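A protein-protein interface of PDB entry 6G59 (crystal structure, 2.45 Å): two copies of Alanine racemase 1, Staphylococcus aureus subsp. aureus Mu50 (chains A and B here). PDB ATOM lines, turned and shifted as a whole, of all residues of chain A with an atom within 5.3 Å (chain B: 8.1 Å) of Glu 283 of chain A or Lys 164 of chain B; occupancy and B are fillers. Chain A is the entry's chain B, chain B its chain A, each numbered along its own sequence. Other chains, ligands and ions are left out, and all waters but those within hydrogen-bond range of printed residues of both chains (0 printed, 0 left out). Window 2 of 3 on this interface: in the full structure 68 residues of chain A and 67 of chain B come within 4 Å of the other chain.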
ATOM      1  N   LYS A 277      26.158  -5.091   9.829  1.00  0.00           N
ATOM      2  CA  LYS A 277      26.454  -6.473   9.422  1.00  0.00           C
ATOM      3  C   LYS A 277      27.806  -6.884   9.962  1.00  0.00           C
ATOM      4  O   LYS A 277      28.698  -6.046  10.099  1.00  0.00           O
ATOM      5  CB  LYS A 277      26.572  -6.596   7.908  1.00  0.00           C
ATOM      6  CG  LYS A 277      25.350  -6.283   7.071  1.00  0.00           C
ATOM      7  CD  LYS A 277      25.526  -6.842   5.669  1.00  0.00           C
ATOM      8  CE  LYS A 277      24.948  -8.243   5.531  1.00  0.00           C
ATOM      9  NZ  LYS A 277      23.499  -8.157   5.194  1.00  0.00           N
ATOM     10  N   THR A 278      27.974  -8.178  10.219  1.00  0.00           N
ATOM     11  CA  THR A 278      29.283  -8.739  10.539  1.00  0.00           C
ATOM     12  C   THR A 278      29.785  -9.497   9.331  1.00  0.00           C
ATOM     13  O   THR A 278      29.094 -10.379   8.833  1.00  0.00           O
ATOM     14  CB  THR A 278      29.190  -9.698  11.727  1.00  0.00           C
ATOM     15  OG1 THR A 278      28.606  -9.004  12.832  1.00  0.00           O
ATOM     16  CG2 THR A 278      30.586 -10.225  12.127  1.00  0.00           C
ATOM     17  N   LEU A 279      30.977  -9.143   8.851  1.00  0.00           N
ATOM     18  CA  LEU A 279      31.628  -9.860   7.754  1.00  0.00           C
ATOM     19  C   LEU A 279      32.597 -10.883   8.320  1.00  0.00           C
ATOM     20  O   LEU A 279      33.375 -10.563   9.227  1.00  0.00           O
ATOM     21  CB  LEU A 279      32.423  -8.898   6.883  1.00  0.00           C
ATOM     22  CG  LEU A 279      31.651  -7.738   6.270  1.00  0.00           C
ATOM     23  CD1 LEU A 279      32.633  -6.751   5.668  1.00  0.00           C
ATOM     24  CD2 LEU A 279      30.634  -8.229   5.251  1.00  0.00           C
ATOM     25  N   GLN A 280      32.558 -12.104   7.789  1.00  0.00           N
ATOM     26  CA  GLN A 280      33.590 -13.108   8.096  1.00  0.00           C
ATOM     27  C   GLN A 280      34.793 -12.906   7.168  1.00  0.00           C
ATOM     28  O   GLN A 280      34.706 -12.209   6.152  1.00  0.00           O
ATOM     29  CB  GLN A 280      33.039 -14.537   7.978  1.00  0.00           C
ATOM     30  CG  GLN A 280      31.983 -14.889   9.021  1.00  0.00           C
ATOM     31  CD  GLN A 280      32.492 -14.740  10.449  1.00  0.00           C
ATOM     32  OE1 GLN A 280      33.375 -15.476  10.879  1.00  0.00           O
ATOM     33  NE2 GLN A 280      31.943 -13.776  11.182  1.00  0.00           N
ATOM     34  N   ALA A 281      35.923 -13.499   7.552  1.00  0.00           N
ATOM     35  CA  ALA A 281      37.152 -13.413   6.770  1.00  0.00           C
ATOM     36  C   ALA A 281      36.909 -13.969   5.375  1.00  0.00           C
ATOM     37  O   ALA A 281      36.414 -15.082   5.233  1.00  0.00           O
ATOM     38  CB  ALA A 281      38.289 -14.157   7.462  1.00  0.00           C
ATOM     39  N   GLY A 282      37.222 -13.163   4.362  1.00  0.00           N
ATOM     40  CA  GLY A 282      36.953 -13.494   2.957  1.00  0.00           C
ATOM     41  C   GLY A 282      35.864 -12.618   2.353  1.00  0.00           C
ATOM     42  O   GLY A 282      35.995 -12.162   1.208  1.00  0.00           O
ATOM     43  N   GLU A 283      34.792 -12.391   3.116  1.00  0.00           N
ATOM     44  CA  GLU A 283      33.623 -11.670   2.621  1.00  0.00           C
ATOM     45  C   GLU A 283      33.928 -10.197   2.365  1.00  0.00           C
ATOM     46  O   GLU A 283      34.721  -9.565   3.078  1.00  0.00           O
ATOM     47  CB  GLU A 283      32.436 -11.807   3.581  1.00  0.00           C
ATOM     48  CG  GLU A 283      31.865 -13.215   3.658  1.00  0.00           C
ATOM     49  CD  GLU A 283      30.797 -13.368   4.731  1.00  0.00           C
ATOM     50  OE1 GLU A 283      30.223 -12.345   5.174  1.00  0.00           O
ATOM     51  OE2 GLU A 283      30.545 -14.522   5.157  1.00  0.00           O
ATOM     52  N   SER A 284      33.353  -9.659   1.287  1.00  0.00           N
ATOM     53  CA  SER A 284      33.600  -8.271   0.858  1.00  0.00           C
ATOM     54  C   SER A 284      32.420  -7.292   0.914  1.00  0.00           C
ATOM     55  O   SER A 284      31.319  -7.647   1.315  1.00  0.00           O
ATOM     56  CB  SER A 284      34.148  -8.262  -0.568  1.00  0.00           C
ATOM     57  OG  SER A 284      33.097  -8.387  -1.504  1.00  0.00           O
ATOM     58  N   VAL A 285      32.677  -6.053   0.492  1.00  0.00           N
ATOM     59  CA  VAL A 285      31.676  -4.990   0.500  1.00  0.00           C
ATOM     60  C   VAL A 285      31.780  -4.031  -0.686  1.00  0.00           C
ATOM     61  O   VAL A 285      32.879  -3.697  -1.126  1.00  0.00           O
ATOM     62  CB  VAL A 285      31.795  -4.126   1.768  1.00  0.00           C
ATOM     63  CG1 VAL A 285      31.269  -4.859   2.984  1.00  0.00           C
ATOM     64  CG2 VAL A 285      33.232  -3.684   1.979  1.00  0.00           C
ATOM     65  N   TYR A 291      37.012  -4.146  -1.047  1.00  0.00           N
ATOM     66  CA  TYR A 291      37.353  -4.401   0.353  1.00  0.00           C
ATOM     67  C   TYR A 291      36.884  -5.744   0.911  1.00  0.00           C
ATOM     68  O   TYR A 291      35.729  -6.121   0.747  1.00  0.00           O
ATOM     69  CB  TYR A 291      36.857  -3.281   1.266  1.00  0.00           C
ATOM     70  CG  TYR A 291      37.331  -3.445   2.690  1.00  0.00           C
ATOM     71  CD1 TYR A 291      36.617  -4.207   3.597  1.00  0.00           C
ATOM     72  CD2 TYR A 291      38.509  -2.862   3.119  1.00  0.00           C
ATOM     73  CE1 TYR A 291      37.052  -4.363   4.896  1.00  0.00           C
ATOM     74  CE2 TYR A 291      38.955  -3.018   4.416  1.00  0.00           C
ATOM     75  CZ  TYR A 291      38.222  -3.767   5.299  1.00  0.00           C
ATOM     76  OH  TYR A 291      38.663  -3.926   6.586  1.00  0.00           O
ATOM     77  N   THR A 292      37.800  -6.444   1.582  1.00  0.00           N
ATOM     78  CA  THR A 292      37.542  -7.731   2.218  1.00  0.00           C
ATOM     79  C   THR A 292      38.021  -7.589   3.650  1.00  0.00           C
ATOM     80  O   THR A 292      39.089  -7.028   3.879  1.00  0.00           O
ATOM     81  CB  THR A 292      38.325  -8.850   1.531  1.00  0.00           C
ATOM     82  OG1 THR A 292      39.706  -8.754   1.896  1.00  0.00           O
ATOM     83  CG2 THR A 292      38.192  -8.732   0.021  1.00  0.00           C
ATOM     84  N   ALA A 293      37.285  -8.121   4.621  1.00  0.00           N
ATOM     85  CA  ALA A 293      37.702  -7.891   6.049  1.00  0.00           C
ATOM     86  C   ALA A 293      38.861  -8.692   6.645  1.00  0.00           C
ATOM     87  O   ALA A 293      39.656  -8.102   7.377  1.00  0.00           O
ATOM     88  CB  ALA A 293      36.489  -7.989   6.960  1.00  0.00           C
ATOM     89  N   PRO B 128      15.184  -4.762   4.522  1.00  0.00           N
ATOM     90  CA  PRO B 128      16.599  -5.140   4.573  1.00  0.00           C
ATOM     91  C   PRO B 128      16.950  -6.199   5.617  1.00  0.00           C
ATOM     92  O   PRO B 128      17.999  -6.804   5.525  1.00  0.00           O
ATOM     93  CB  PRO B 128      17.275  -3.820   4.927  1.00  0.00           C
ATOM     94  CG  PRO B 128      16.270  -3.106   5.770  1.00  0.00           C
ATOM     95  CD  PRO B 128      14.915  -3.559   5.330  1.00  0.00           C
ATOM     96  N   SER B 129      16.079  -6.409   6.597  1.00  0.00           N
ATOM     97  CA  SER B 129      16.370  -7.273   7.741  1.00  0.00           C
ATOM     98  C   SER B 129      15.091  -7.657   8.472  1.00  0.00           C
ATOM     99  O   SER B 129      14.056  -7.010   8.302  1.00  0.00           O
ATOM    100  CB  SER B 129      17.296  -6.540   8.730  1.00  0.00           C
ATOM    101  OG  SER B 129      16.607  -5.459   9.326  1.00  0.00           O
ATOM    102  N   LYS B 153      14.891  -7.456   0.178  1.00  0.00           N
ATOM    103  CA  LYS B 153      16.239  -7.354  -0.377  1.00  0.00           C
ATOM    104  C   LYS B 153      17.046  -8.542   0.126  1.00  0.00           C
ATOM    105  O   LYS B 153      17.092  -8.775   1.334  1.00  0.00           O
ATOM    106  CB  LYS B 153      16.886  -6.045   0.065  1.00  0.00           C
ATOM    107  CG  LYS B 153      18.342  -5.815  -0.330  1.00  0.00           C
ATOM    108  CD  LYS B 153      18.508  -5.395  -1.779  1.00  0.00           C
ATOM    109  CE  LYS B 153      19.956  -4.977  -2.076  1.00  0.00           C
ATOM    110  NZ  LYS B 153      20.865  -6.141  -2.383  1.00  0.00           N
ATOM    111  N   LEU B 154      17.655  -9.288  -0.803  1.00  0.00           N
ATOM    112  CA  LEU B 154      18.620 -10.349  -0.491  1.00  0.00           C
ATOM    113  C   LEU B 154      20.051  -9.913  -0.788  1.00  0.00           C
ATOM    114  O   LEU B 154      20.336  -9.421  -1.872  1.00  0.00           O
ATOM    115  CB  LEU B 154      18.318 -11.604  -1.306  1.00  0.00           C
ATOM    116  CG  LEU B 154      16.933 -12.201  -1.104  1.00  0.00           C
ATOM    117  CD1 LEU B 154      16.849 -13.523  -1.843  1.00  0.00           C
ATOM    118  CD2 LEU B 154      16.597 -12.427   0.363  1.00  0.00           C
ATOM    119  N   ASP B 155      20.927 -10.075   0.204  1.00  0.00           N
ATOM    120  CA  ASP B 155      22.370  -9.915   0.050  1.00  0.00           C
ATOM    121  C   ASP B 155      22.920 -11.243  -0.438  1.00  0.00           C
ATOM    122  O   ASP B 155      22.931 -12.242   0.299  1.00  0.00           O
ATOM    123  CB  ASP B 155      23.024  -9.515   1.392  1.00  0.00           C
ATOM    124  CG  ASP B 155      24.570  -9.493   1.336  1.00  0.00           C
ATOM    125  OD1 ASP B 155      25.157  -9.530   0.228  1.00  0.00           O
ATOM    126  OD2 ASP B 155      25.215  -9.432   2.404  1.00  0.00           O
ATOM    127  N   THR B 156      23.382 -11.238  -1.686  1.00  0.00           N
ATOM    128  CA  THR B 156      23.917 -12.433  -2.318  1.00  0.00           C
ATOM    129  C   THR B 156      25.437 -12.386  -2.504  1.00  0.00           C
ATOM    130  O   THR B 156      25.974 -13.237  -3.196  1.00  0.00           O
ATOM    131  CB  THR B 156      23.242 -12.647  -3.675  1.00  0.00           C
ATOM    132  OG1 THR B 156      23.368 -11.455  -4.458  1.00  0.00           O
ATOM    133  CG2 THR B 156      21.783 -12.962  -3.479  1.00  0.00           C
ATOM    134  N   GLY B 157      26.079 -11.472  -1.786  1.00  0.00           N
ATOM    135  CA  GLY B 157      27.507 -11.251  -1.849  1.00  0.00           C
ATOM    136  C   GLY B 157      27.954  -9.799  -1.956  1.00  0.00           C
ATOM    137  O   GLY B 157      29.125  -9.508  -1.765  1.00  0.00           O
ATOM    138  N   MET B 158      27.030  -8.882  -2.219  1.00  0.00           N
ATOM    139  CA  MET B 158      27.367  -7.457  -2.304  1.00  0.00           C
ATOM    140  C   MET B 158      27.882  -6.925  -0.968  1.00  0.00           C
ATOM    141  O   MET B 158      28.775  -6.089  -0.932  1.00  0.00           O
ATOM    142  CB  MET B 158      26.185  -6.625  -2.797  1.00  0.00           C
ATOM    143  CG  MET B 158      26.345  -5.121  -2.621  1.00  0.00           C
ATOM    144  SD  MET B 158      27.177  -4.237  -3.957  1.00  0.00           S
ATOM    145  CE  MET B 158      25.879  -4.137  -5.173  1.00  0.00           C
ATOM    146  N   GLY B 159      27.299  -7.397   0.127  1.00  0.00           N
ATOM    147  CA  GLY B 159      27.712  -6.988   1.457  1.00  0.00           C
ATOM    148  C   GLY B 159      27.111  -5.690   1.945  1.00  0.00           C
ATOM    149  O   GLY B 159      27.499  -5.170   2.975  1.00  0.00           O
ATOM    150  N   ARG B 160      26.142  -5.179   1.208  1.00  0.00           N
ATOM    151  CA  ARG B 160      25.482  -3.932   1.540  1.00  0.00           C
ATOM    152  C   ARG B 160      24.202  -4.289   2.283  1.00  0.00           C
ATOM    153  O   ARG B 160      24.242  -5.015   3.267  1.00  0.00           O
ATOM    154  CB  ARG B 160      25.178  -3.196   0.241  1.00  0.00           C
ATOM    155  CG  ARG B 160      25.040  -1.676   0.296  1.00  0.00           C
ATOM    156  CD  ARG B 160      24.885  -1.072  -1.104  1.00  0.00           C
ATOM    157  NE  ARG B 160      24.611  -2.081  -2.132  1.00  0.00           N
ATOM    158  CZ  ARG B 160      23.547  -2.877  -2.142  1.00  0.00           C
ATOM    159  NH1 ARG B 160      22.625  -2.776  -1.202  1.00  0.00           N
ATOM    160  NH2 ARG B 160      23.406  -3.770  -3.097  1.00  0.00           N
ATOM    161  N   LEU B 161      23.077  -3.753   1.837  1.00  0.00           N
ATOM    162  CA  LEU B 161      21.787  -4.039   2.441  1.00  0.00           C
ATOM    163  C   LEU B 161      21.294  -5.439   2.107  1.00  0.00           C
ATOM    164  O   LEU B 161      21.738  -6.046   1.144  1.00  0.00           O
ATOM    165  CB  LEU B 161      20.742  -3.029   1.964  1.00  0.00           C
ATOM    166  CG  LEU B 161      20.817  -1.592   2.454  1.00  0.00           C
ATOM    167  CD1 LEU B 161      19.596  -0.817   1.983  1.00  0.00           C
ATOM    168  CD2 LEU B 161      20.933  -1.542   3.963  1.00  0.00           C
ATOM    169  N   GLY B 162      20.384  -5.951   2.921  1.00  0.00           N
ATOM    170  CA  GLY B 162      19.786  -7.245   2.664  1.00  0.00           C
ATOM    171  C   GLY B 162      19.979  -8.412   3.606  1.00  0.00           C
ATOM    172  O   GLY B 162      20.848  -8.416   4.463  1.00  0.00           O
ATOM    173  N   ILE B 163      19.129  -9.412   3.408  1.00  0.00           N
ATOM    174  CA  ILE B 163      19.119 -10.641   4.172  1.00  0.00           C
ATOM    175  C   ILE B 163      20.017 -11.614   3.454  1.00  0.00           C
ATOM    176  O   ILE B 163      19.923 -11.762   2.242  1.00  0.00           O
ATOM    177  CB  ILE B 163      17.690 -11.209   4.279  1.00  0.00           C
ATOM    178  CG1 ILE B 163      16.836 -10.285   5.164  1.00  0.00           C
ATOM    179  CG2 ILE B 163      17.712 -12.640   4.837  1.00  0.00           C
ATOM    180  CD1 ILE B 163      15.344 -10.390   4.949  1.00  0.00           C
ATOM    181  N   LYS B 164      20.897 -12.276   4.190  1.00  0.00           N
ATOM    182  CA  LYS B 164      21.884 -13.120   3.556  1.00  0.00           C
ATOM    183  C   LYS B 164      21.650 -14.612   3.721  1.00  0.00           C
ATOM    184  O   LYS B 164      22.251 -15.392   2.997  1.00  0.00           O
ATOM    185  CB  LYS B 164      23.293 -12.688   3.962  1.00  0.00           C
ATOM    186  CG  LYS B 164      23.790 -13.163   5.321  1.00  0.00           C
ATOM    187  CD  LYS B 164      24.966 -12.327   5.822  1.00  0.00           C
ATOM    188  CE  LYS B 164      26.019 -12.061   4.741  1.00  0.00           C
ATOM    189  NZ  LYS B 164      27.356 -11.708   5.296  1.00  0.00           N
ATOM    190  N   ASP B 165      20.756 -14.992   4.634  1.00  0.00           N
ATOM    191  CA  ASP B 165      20.508 -16.388   4.936  1.00  0.00           C
ATOM    192  C   ASP B 165      19.051 -16.771   4.676  1.00  0.00           C
ATOM    193  O   ASP B 165      18.120 -15.985   4.841  1.00  0.00           O
ATOM    194  CB  ASP B 165      20.912 -16.703   6.380  1.00  0.00           C
ATOM    195  CG  ASP B 165      20.017 -16.010   7.420  1.00  0.00           C
ATOM    196  OD1 ASP B 165      19.963 -14.751   7.451  1.00  0.00           O
ATOM    197  OD2 ASP B 165      19.374 -16.744   8.194  1.00  0.00           O
ATOM    198  N   THR B 166      18.876 -18.013   4.262  1.00  0.00           N
ATOM    199  CA  THR B 166      17.581 -18.521   3.847  1.00  0.00           C
ATOM    200  C   THR B 166      16.565 -18.591   4.991  1.00  0.00           C
ATOM    201  O   THR B 166      15.403 -18.258   4.776  1.00  0.00           O
ATOM    202  CB  THR B 166      17.757 -19.885   3.143  1.00  0.00           C
ATOM    203  OG1 THR B 166      18.591 -19.674   1.988  1.00  0.00           O
ATOM    204  CG2 THR B 166      16.443 -20.461   2.670  1.00  0.00           C
ATOM    205  N   ASN B 167      16.989 -18.997   6.189  1.00  0.00           N
ATOM    206  CA  ASN B 167      16.059 -19.107   7.326  1.00  0.00           C
ATOM    207  C   ASN B 167      15.402 -17.774   7.661  1.00  0.00           C
ATOM    208  O   ASN B 167      14.185 -17.721   7.910  1.00  0.00           O
ATOM    209  CB  ASN B 167      16.738 -19.640   8.605  1.00  0.00           C
ATOM    210  CG  ASN B 167      17.215 -21.105   8.517  1.00  0.00           C
ATOM    211  OD1 ASN B 167      16.991 -21.827   7.538  1.00  0.00           O
ATOM    212  ND2 ASN B 167      17.913 -21.535   9.554  1.00  0.00           N
ATOM    213  N   THR B 168      16.206 -16.708   7.660  1.00  0.00           N
ATOM    214  CA  THR B 168      15.693 -15.361   7.927  1.00  0.00           C
ATOM    215  C   THR B 168      14.727 -14.902   6.841  1.00  0.00           C
ATOM    216  O   THR B 168      13.704 -14.299   7.129  1.00  0.00           O
ATOM    217  CB  THR B 168      16.846 -14.345   8.062  1.00  0.00           C
ATOM    218  OG1 THR B 168      17.705 -14.749   9.148  1.00  0.00           O
ATOM    219  CG2 THR B 168      16.324 -12.917   8.312  1.00  0.00           C
ATOM    220  N   TYR B 169      15.065 -15.184   5.592  1.00  0.00           N
ATOM    221  CA  TYR B 169      14.182 -14.909   4.448  1.00  0.00           C
ATOM    222  C   TYR B 169      12.820 -15.548   4.635  1.00  0.00           C
ATOM    223  O   TYR B 169      11.795 -14.893   4.453  1.00  0.00           O
ATOM    224  CB  TYR B 169      14.840 -15.422   3.160  1.00  0.00           C
ATOM    225  CG  TYR B 169      14.059 -15.246   1.891  1.00  0.00           C
ATOM    226  CD1 TYR B 169      13.560 -14.004   1.516  1.00  0.00           C
ATOM    227  CD2 TYR B 169      13.865 -16.330   1.023  1.00  0.00           C
ATOM    228  CE1 TYR B 169      12.848 -13.860   0.319  1.00  0.00           C
ATOM    229  CE2 TYR B 169      13.186 -16.180  -0.187  1.00  0.00           C
ATOM    230  CZ  TYR B 169      12.668 -14.951  -0.521  1.00  0.00           C
ATOM    231  OH  TYR B 169      11.972 -14.799  -1.688  1.00  0.00           O
ATOM    232  N   MET B 200      31.942 -13.279 -10.307  1.00  0.00           N
ATOM    233  CA  MET B 200      31.148 -12.925  -9.132  1.00  0.00           C
ATOM    234  C   MET B 200      29.668 -12.749  -9.470  1.00  0.00           C
ATOM    235  O   MET B 200      28.813 -13.186  -8.718  1.00  0.00           O
ATOM    236  CB  MET B 200      31.687 -11.671  -8.443  1.00  0.00           C
ATOM    237  CG  MET B 200      31.158 -11.508  -7.026  1.00  0.00           C
ATOM    238  SD  MET B 200      31.644  -9.935  -6.306  1.00  0.00           S
ATOM    239  CE  MET B 200      30.883 -10.121  -4.692  1.00  0.00           C
ATOM    240  N   ARG B 207      23.139 -17.866  -6.419  1.00  0.00           N
ATOM    241  CA  ARG B 207      22.793 -17.754  -5.000  1.00  0.00           C
ATOM    242  C   ARG B 207      21.385 -17.176  -4.822  1.00  0.00           C
ATOM    243  O   ARG B 207      20.602 -17.661  -4.001  1.00  0.00           O
ATOM    244  CB  ARG B 207      23.840 -16.876  -4.283  1.00  0.00           C
ATOM    245  CG  ARG B 207      23.582 -16.556  -2.815  1.00  0.00           C
ATOM    246  CD  ARG B 207      23.516 -17.804  -1.955  1.00  0.00           C
ATOM    247  NE  ARG B 207      23.051 -17.460  -0.613  1.00  0.00           N
ATOM    248  CZ  ARG B 207      22.718 -18.331   0.339  1.00  0.00           C
ATOM    249  NH1 ARG B 207      22.894 -19.640   0.161  1.00  0.00           N
ATOM    250  NH2 ARG B 207      22.286 -17.902   1.527  1.00  0.00           N
ATOM    251  N   MET B 211      18.143 -19.137  -3.012  1.00  0.00           N
ATOM    252  CA  MET B 211      17.381 -18.632  -1.879  1.00  0.00           C
ATOM    253  C   MET B 211      15.893 -18.524  -2.240  1.00  0.00           C
ATOM    254  O   MET B 211      15.023 -18.998  -1.502  1.00  0.00           O
ATOM    255  CB  MET B 211      17.925 -17.269  -1.437  1.00  0.00           C
ATOM    256  CG  MET B 211      19.331 -17.341  -0.833  1.00  0.00           C
ATOM    257  SD  MET B 211      20.011 -15.711  -0.447  1.00  0.00           S
ATOM    258  CE  MET B 211      19.192 -15.330   1.127  1.00  0.00           C
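Lys 277 of chain A touches Gly 159 of chain B (CD to O, 3.7 Å).
Arg 160 of chain B touches Lys 277 of chain A (O to CD, 3.3 Å).
Ser 284 of chain A touches Met 158 of chain B (O to O, 3.7 Å).
Ser 284 of chain A touches Gly 159 of chain B (O to CA, 3.7 Å).
CA of Val 285 of chain A touches O of Met 158 of chain B (3.4 Å).
CG1 of Val 285 of chain A touches O of Gly 159 of chain B (3.8 Å).
Leu 279 of chain A touches none of the printed residues of chain B.
No residue of chain B comes within 4 Å of Gly 282 of chain A.
Glu 283 of chain A touches one residue of chain B.
Of the printed residues of chain B, Ser 284 of chain A touches Met 158 (3.7 Å) and Gly 159 (3.7 Å).
Printed residues of chain B within 4 Å of Val 285 of chain A: Met 158 and Gly 159.
Printed residues of chain A within 4 Å of Asp 155 of chain B: Lys 277 (3.4 Å).
Of the printed residues of chain A, Gly 159 of chain B touches Lys 277 (3.7 Å), Ser 284 (3.7 Å) and Val 285 (3.8 Å).
Lys 164 of chain B touches just one residue of chain A: Glu 283.
Thr 168 of chain B touches none of the printed residues of chain A.
The nearest residue of chain A that does not touch Lys 164 of chain B is Lys 277 of chain A (4.04 Å).
No position is printed for both chains.
NZ of Lys 164 of chain B is in salt-bridge range of OE1 of Glu 283 of chain A (2.9 Å).
The side-chain carboxylate (OD2) of Asp 155 of chain B is in salt-bridge range of the side-chain amino group (NZ) of Lys 277 of chain A, 3.5 Å away.
O of Gly 162 of chain B lies within hydrogen-bond range of NZ of Lys 277 of chain A (2.8 Å).
Printed residues of chain A that touch a printed residue of chain B: Lys 277, Glu 283, Ser 284 and Val 285.
Hydrophobic or aromatic side chains of chain A that line the printed part of chain B: Val 285.
Of the 22 printed residues of chain B, 6 touch a printed residue of chain A.
Among the printed residues, 9 pairs touch across the chains.
OD1 of Asp 155 of chain B sits at hydrogen-bond distance from N of Gly 157 of chain B, at 2.9 Å.
The backbone NH of Asp 155 of chain B is in hydrogen-bond range of the backbone carbonyl oxygen of Ile 163 of chain B (2.8 Å).
The side-chain carboxylate (OD1) of Asp 155 of chain B sits at hydrogen-bond distance from the backbone NH (N) of Met 158 of chain B, at 3.1 Å.
The side-chain carboxylate of Asp 155 of chain B sits at hydrogen-bond distance from the backbone NH of Gly 159 of chain B, 3.0 Å away.
N of Val 285 of chain A sits at hydrogen-bond distance from O of Tyr 291 of chain A (3.1 Å).
The backbone carbonyl oxygen of Lys 164 of chain B is in hydrogen-bond range of the guanidinium group of Arg 207 of chain B (2.9 Å).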
